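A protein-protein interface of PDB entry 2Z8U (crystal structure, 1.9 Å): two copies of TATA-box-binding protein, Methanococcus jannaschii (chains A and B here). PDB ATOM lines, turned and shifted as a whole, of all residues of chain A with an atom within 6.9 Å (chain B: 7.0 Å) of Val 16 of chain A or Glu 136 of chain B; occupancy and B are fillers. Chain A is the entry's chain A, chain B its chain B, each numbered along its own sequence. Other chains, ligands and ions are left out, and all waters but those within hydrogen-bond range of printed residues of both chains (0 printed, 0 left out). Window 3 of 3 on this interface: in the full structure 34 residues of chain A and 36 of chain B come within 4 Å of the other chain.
Of the 7 printed residues of chain B, 4 touch a printed residue of chain A. Of the 14 printed residues of chain A, 5 touch a printed residue of chain B. Hydrophobic or aromatic side chains of chain A that line the printed part of chain B: Val 16 and Val 110. Among the printed residues, 7 pairs touch across the chains. Among the printed residues, no Asp or Glu carboxylate lies within 4 Å of a Lys or Arg side-chain nitrogen of the other chain.
Of chain B, only Glu 134 (3.2 Å) and Glu 136 (3.6 Å) come within 4 Å of Val 16 of chain A. Of chain A, only Val 16 comes within 4 Å of Glu 136 of chain B. Of the printed residues of chain A, Gln 137 of chain B touches Thr 112 (3.5 Å) and Lys 159 (2.8 Å). Printed residues of chain B within 4 Å of Val 110 of chain A: Glu 134. The nearest residue of chain B that does not touch Val 16 of chain A is Gln 137 of chain B (4.2 Å).
No position is printed for both chains. Of the 7 pairs that touch across the chains among the printed residues, none has its exchanged pair printed and touching as well.
Val 16 of chain A touches Glu 134 of chain B (CG1 to OE1, 3.2 Å). Glu 136 of chain B touches Val 16 of chain A (OE1 to CG1, 3.6 Å). ND2 of Asn 17 of chain A touches O of Tyr 133 of chain B, 3.9 Å away. CG2 of Val 110 of chain A touches CG of Glu 134 of chain B (3.9 Å). Thr 112 of chain A touches Gln 137 of chain B.
The side-chain carboxylate (OE2) of Glu 134 of chain B is in hydrogen-bond range of the side-chain amide nitrogen (ND2) of Asn 17 of chain A (2.9 Å). The side-chain amino group (NZ) of Lys 159 of chain A lies within hydrogen-bond range of the backbone carbonyl oxygen (O) of Gln 137 of chain B (2.8 Å).
The backbone carbonyl oxygen (O) of Lys 14 of chain A sits at hydrogen-bond distance from the backbone NH (N) of Thr 112 of chain A, 2.8 Å away. The backbone NH of Val 16 of chain A lies within hydrogen-bond range of the backbone carbonyl oxygen of Val 110 of chain A, at 2.8 Å. O of Asn 17 of chain A lies within hydrogen-bond range of N of Val 110 of chain A, at 3.1 Å. The side-chain carboxylate (OE1) of Glu 136 of chain B lies within hydrogen-bond range of the side-chain amide nitrogen (NE2) of Gln 137 of chain B, at 2.8 Å.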
ATOM      1  N   LYS A  14      26.405  -2.812  19.639  1.00  0.00           N
ATOM      2  CA  LYS A  14      25.443  -1.806  20.091  1.00  0.00           C
ATOM      3  C   LYS A  14      26.183  -0.724  20.896  1.00  0.00           C
ATOM      4  O   LYS A  14      26.965  -1.039  21.803  1.00  0.00           O
ATOM      5  CB  LYS A  14      24.341  -2.464  20.928  1.00  0.00           C
ATOM      6  CG  LYS A  14      23.541  -1.515  21.817  1.00  0.00           C
ATOM      7  CD  LYS A  14      22.118  -2.015  22.099  1.00  0.00           C
ATOM      8  CE  LYS A  14      21.409  -1.077  23.087  1.00  0.00           C
ATOM      9  NZ  LYS A  14      19.965  -1.423  23.305  1.00  0.00           N
ATOM     10  N   ILE A  15      25.961   0.540  20.543  1.00  0.00           N
ATOM     11  CA  ILE A  15      26.512   1.649  21.336  1.00  0.00           C
ATOM     12  C   ILE A  15      25.530   1.910  22.468  1.00  0.00           C
ATOM     13  O   ILE A  15      24.346   2.095  22.218  1.00  0.00           O
ATOM     14  CB  ILE A  15      26.777   2.932  20.494  1.00  0.00           C
ATOM     15  CG1 ILE A  15      27.727   2.622  19.329  1.00  0.00           C
ATOM     16  CG2 ILE A  15      27.361   4.049  21.384  1.00  0.00           C
ATOM     17  CD1 ILE A  15      29.024   1.926  19.733  1.00  0.00           C
ATOM     18  N   VAL A  16      26.010   1.838  23.709  1.00  0.00           N
ATOM     19  CA  VAL A  16      25.123   1.961  24.884  1.00  0.00           C
ATOM     20  C   VAL A  16      25.205   3.356  25.511  1.00  0.00           C
ATOM     21  O   VAL A  16      24.208   3.887  26.010  1.00  0.00           O
ATOM     22  CB  VAL A  16      25.364   0.827  25.927  1.00  0.00           C
ATOM     23  CG1 VAL A  16      24.519   1.040  27.171  1.00  0.00           C
ATOM     24  CG2 VAL A  16      25.018  -0.531  25.315  1.00  0.00           C
ATOM     25  N   ASN A  17      26.385   3.965  25.453  1.00  0.00           N
ATOM     26  CA  ASN A  17      26.523   5.348  25.853  1.00  0.00           C
ATOM     27  C   ASN A  17      27.693   5.997  25.147  1.00  0.00           C
ATOM     28  O   ASN A  17      28.576   5.314  24.616  1.00  0.00           O
ATOM     29  CB  ASN A  17      26.546   5.520  27.395  1.00  0.00           C
ATOM     30  CG  ASN A  17      27.931   5.484  27.991  1.00  0.00           C
ATOM     31  OD1 ASN A  17      28.852   6.125  27.493  1.00  0.00           O
ATOM     32  ND2 ASN A  17      28.065   4.801  29.137  1.00  0.00           N
ATOM     33  N   VAL A  18      27.649   7.317  25.071  1.00  0.00           N
ATOM     34  CA  VAL A  18      28.765   8.072  24.582  1.00  0.00           C
ATOM     35  C   VAL A  18      29.082   9.130  25.636  1.00  0.00           C
ATOM     36  O   VAL A  18      28.203   9.539  26.433  1.00  0.00           O
ATOM     37  CB  VAL A  18      28.496   8.698  23.178  1.00  0.00           C
ATOM     38  CG1 VAL A  18      28.268   7.601  22.097  1.00  0.00           C
ATOM     39  CG2 VAL A  18      27.302   9.623  23.213  1.00  0.00           C
ATOM     40  N   GLY A  73      25.843  10.196  29.551  1.00  0.00           N
ATOM     41  CA  GLY A  73      24.471   9.694  29.606  1.00  0.00           C
ATOM     42  C   GLY A  73      23.754   9.535  28.276  1.00  0.00           C
ATOM     43  O   GLY A  73      22.769   8.789  28.186  1.00  0.00           O
ATOM     44  N   ALA A  74      24.240  10.211  27.235  1.00  0.00           N
ATOM     45  CA  ALA A  74      23.633  10.098  25.898  1.00  0.00           C
ATOM     46  C   ALA A  74      23.872   8.735  25.229  1.00  0.00           C
ATOM     47  O   ALA A  74      24.966   8.152  25.334  1.00  0.00           O
ATOM     48  CB  ALA A  74      24.123  11.205  24.993  1.00  0.00           C
ATOM     49  N   LYS A  75      22.856   8.267  24.510  1.00  0.00           N
ATOM     50  CA  LYS A  75      22.917   7.005  23.769  1.00  0.00           C
ATOM     51  C   LYS A  75      23.741   7.174  22.506  1.00  0.00           C
ATOM     52  O   LYS A  75      24.278   6.195  21.971  1.00  0.00           O
ATOM     53  CB  LYS A  75      21.507   6.516  23.398  1.00  0.00           C
ATOM     54  CG  LYS A  75      20.688   6.055  24.590  1.00  0.00           C
ATOM     55  CD  LYS A  75      19.448   5.305  24.182  1.00  0.00           C
ATOM     56  CE  LYS A  75      18.367   5.440  25.247  1.00  0.00           C
ATOM     57  NZ  LYS A  75      17.093   4.807  24.818  1.00  0.00           N
ATOM     58  N   SER A  76      23.851   8.417  22.034  1.00  0.00           N
ATOM     59  CA  SER A  76      24.508   8.704  20.760  1.00  0.00           C
ATOM     60  C   SER A  76      25.043  10.123  20.709  1.00  0.00           C
ATOM     61  O   SER A  76      24.632  10.971  21.498  1.00  0.00           O
ATOM     62  CB  SER A  76      23.518   8.504  19.598  1.00  0.00           C
ATOM     63  OG  SER A  76      22.457   9.448  19.656  1.00  0.00           O
ATOM     64  N   MET A 109      33.055   5.874  24.616  1.00  0.00           N
ATOM     65  CA  MET A 109      31.837   5.079  24.451  1.00  0.00           C
ATOM     66  C   MET A 109      31.886   3.800  25.250  1.00  0.00           C
ATOM     67  O   MET A 109      32.978   3.295  25.627  1.00  0.00           O
ATOM     68  CB  MET A 109      31.656   4.655  23.004  1.00  0.00           C
ATOM     69  CG  MET A 109      31.669   5.744  22.004  1.00  0.00           C
ATOM     70  SD  MET A 109      31.888   4.991  20.402  1.00  0.00           S
ATOM     71  CE  MET A 109      31.612   6.394  19.341  1.00  0.00           C
ATOM     72  N   VAL A 110      30.697   3.260  25.489  1.00  0.00           N
ATOM     73  CA  VAL A 110      30.561   1.881  25.865  1.00  0.00           C
ATOM     74  C   VAL A 110      29.827   1.230  24.688  1.00  0.00           C
ATOM     75  O   VAL A 110      28.774   1.731  24.267  1.00  0.00           O
ATOM     76  CB  VAL A 110      29.778   1.702  27.183  1.00  0.00           C
ATOM     77  CG1 VAL A 110      29.380   0.279  27.381  1.00  0.00           C
ATOM     78  CG2 VAL A 110      30.623   2.175  28.393  1.00  0.00           C
ATOM     79  N   ALA A 111      30.426   0.171  24.138  1.00  0.00           N
ATOM     80  CA  ALA A 111      29.785  -0.660  23.125  1.00  0.00           C
ATOM     81  C   ALA A 111      29.632  -2.070  23.696  1.00  0.00           C
ATOM     82  O   ALA A 111      30.459  -2.506  24.491  1.00  0.00           O
ATOM     83  CB  ALA A 111      30.608  -0.684  21.846  1.00  0.00           C
ATOM     84  N   THR A 112      28.549  -2.761  23.331  1.00  0.00           N
ATOM     85  CA  THR A 112      28.340  -4.135  23.778  1.00  0.00           C
ATOM     86  C   THR A 112      28.132  -5.049  22.580  1.00  0.00           C
ATOM     87  O   THR A 112      27.631  -4.635  21.548  1.00  0.00           O
ATOM     88  CB  THR A 112      27.117  -4.283  24.684  1.00  0.00           C
ATOM     89  OG1 THR A 112      25.959  -3.824  23.974  1.00  0.00           O
ATOM     90  CG2 THR A 112      27.290  -3.498  25.986  1.00  0.00           C
ATOM     91  N   LYS A 159      28.828 -12.175  26.554  1.00  0.00           N
ATOM     92  CA  LYS A 159      28.687 -10.727  26.477  1.00  0.00           C
ATOM     93  C   LYS A 159      30.032 -10.033  26.638  1.00  0.00           C
ATOM     94  O   LYS A 159      30.835 -10.395  27.497  1.00  0.00           O
ATOM     95  CB  LYS A 159      27.718 -10.222  27.548  1.00  0.00           C
ATOM     96  CG  LYS A 159      27.672  -8.685  27.685  1.00  0.00           C
ATOM     97  CD  LYS A 159      26.602  -8.268  28.687  1.00  0.00           C
ATOM     98  CE  LYS A 159      27.040  -7.030  29.459  1.00  0.00           C
ATOM     99  NZ  LYS A 159      26.247  -6.924  30.728  1.00  0.00           N
ATOM    100  N   TYR B 133      31.221   4.216  33.125  1.00  0.00           N
ATOM    101  CA  TYR B 133      30.367   3.653  34.149  1.00  0.00           C
ATOM    102  C   TYR B 133      29.035   3.379  33.503  1.00  0.00           C
ATOM    103  O   TYR B 133      28.394   4.303  32.958  1.00  0.00           O
ATOM    104  CB  TYR B 133      30.232   4.633  35.311  1.00  0.00           C
ATOM    105  CG  TYR B 133      29.339   4.174  36.433  1.00  0.00           C
ATOM    106  CD1 TYR B 133      29.582   2.979  37.092  1.00  0.00           C
ATOM    107  CD2 TYR B 133      28.263   4.956  36.855  1.00  0.00           C
ATOM    108  CE1 TYR B 133      28.760   2.552  38.147  1.00  0.00           C
ATOM    109  CE2 TYR B 133      27.441   4.545  37.906  1.00  0.00           C
ATOM    110  CZ  TYR B 133      27.694   3.341  38.540  1.00  0.00           C
ATOM    111  OH  TYR B 133      26.890   2.922  39.587  1.00  0.00           O
ATOM    112  N   GLU B 134      28.640   2.111  33.521  1.00  0.00           N
ATOM    113  CA  GLU B 134      27.360   1.673  32.982  1.00  0.00           C
ATOM    114  C   GLU B 134      26.872   0.529  33.835  1.00  0.00           C
ATOM    115  O   GLU B 134      27.072  -0.628  33.454  1.00  0.00           O
ATOM    116  CB  GLU B 134      27.533   1.166  31.547  1.00  0.00           C
ATOM    117  CG  GLU B 134      27.330   2.187  30.500  1.00  0.00           C
ATOM    118  CD  GLU B 134      25.873   2.583  30.340  1.00  0.00           C
ATOM    119  OE1 GLU B 134      24.976   1.706  30.285  1.00  0.00           O
ATOM    120  OE2 GLU B 134      25.632   3.789  30.271  1.00  0.00           O
ATOM    121  N   PRO B 135      26.256   0.837  35.004  1.00  0.00           N
ATOM    122  CA  PRO B 135      25.910  -0.220  35.967  1.00  0.00           C
ATOM    123  C   PRO B 135      25.020  -1.344  35.421  1.00  0.00           C
ATOM    124  O   PRO B 135      25.078  -2.458  35.924  1.00  0.00           O
ATOM    125  CB  PRO B 135      25.229   0.538  37.128  1.00  0.00           C
ATOM    126  CG  PRO B 135      24.959   1.904  36.636  1.00  0.00           C
ATOM    127  CD  PRO B 135      25.900   2.182  35.502  1.00  0.00           C
ATOM    128  N   GLU B 136      24.231  -1.065  34.388  1.00  0.00           N
ATOM    129  CA  GLU B 136      23.406  -2.099  33.752  1.00  0.00           C
ATOM    130  C   GLU B 136      24.231  -3.086  32.919  1.00  0.00           C
ATOM    131  O   GLU B 136      23.751  -4.174  32.588  1.00  0.00           O
ATOM    132  CB  GLU B 136      22.310  -1.469  32.885  1.00  0.00           C
ATOM    133  CG  GLU B 136      22.802  -0.324  32.008  1.00  0.00           C
ATOM    134  CD  GLU B 136      22.005  -0.164  30.745  1.00  0.00           C
ATOM    135  OE1 GLU B 136      22.497  -0.612  29.686  1.00  0.00           O
ATOM    136  OE2 GLU B 136      20.883   0.399  30.808  1.00  0.00           O
ATOM    137  N   GLN B 137      25.463  -2.706  32.577  1.00  0.00           N
ATOM    138  CA  GLN B 137      26.305  -3.533  31.716  1.00  0.00           C
ATOM    139  C   GLN B 137      27.453  -4.190  32.484  1.00  0.00           C
ATOM    140  O   GLN B 137      27.941  -5.248  32.102  1.00  0.00           O
ATOM    141  CB  GLN B 137      26.835  -2.728  30.522  1.00  0.00           C
ATOM    142  CG  GLN B 137      25.758  -2.262  29.516  1.00  0.00           C
ATOM    143  CD  GLN B 137      24.867  -3.386  29.001  1.00  0.00           C
ATOM    144  OE1 GLN B 137      25.338  -4.487  28.712  1.00  0.00           O
ATOM    145  NE2 GLN B 137      23.571  -3.112  28.885  1.00  0.00           N
ATOM    146  N   PHE B 138      27.888  -3.558  33.559  1.00  0.00           N
ATOM    147  CA  PHE B 138      28.971  -4.086  34.375  1.00  0.00           C
ATOM    148  C   PHE B 138      29.036  -3.341  35.695  1.00  0.00           C
ATOM    149  O   PHE B 138      28.738  -2.146  35.754  1.00  0.00           O
ATOM    150  CB  PHE B 138      30.333  -4.014  33.632  1.00  0.00           C
ATOM    151  CG  PHE B 138      30.720  -2.629  33.182  1.00  0.00           C
ATOM    152  CD1 PHE B 138      31.577  -1.850  33.947  1.00  0.00           C
ATOM    153  CD2 PHE B 138      30.240  -2.103  31.979  1.00  0.00           C
ATOM    154  CE1 PHE B 138      31.928  -0.558  33.538  1.00  0.00           C
ATOM    155  CE2 PHE B 138      30.596  -0.805  31.564  1.00  0.00           C
ATOM    156  CZ  PHE B 138      31.439  -0.042  32.338  1.00  0.00           C
ATOM    157  N   PRO B 139      29.458  -4.034  36.763  1.00  0.00           N
ATOM    158  CA  PRO B 139      29.558  -3.358  38.037  1.00  0.00           C
ATOM    159  C   PRO B 139      30.873  -2.560  38.078  1.00  0.00           C
ATOM    160  O   PRO B 139      31.879  -3.016  37.529  1.00  0.00           O
ATOM    161  CB  PRO B 139      29.616  -4.531  39.026  1.00  0.00           C
ATOM    162  CG  PRO B 139      30.342  -5.578  38.296  1.00  0.00           C
ATOM    163  CD  PRO B 139      29.879  -5.452  36.861  1.00  0.00           C
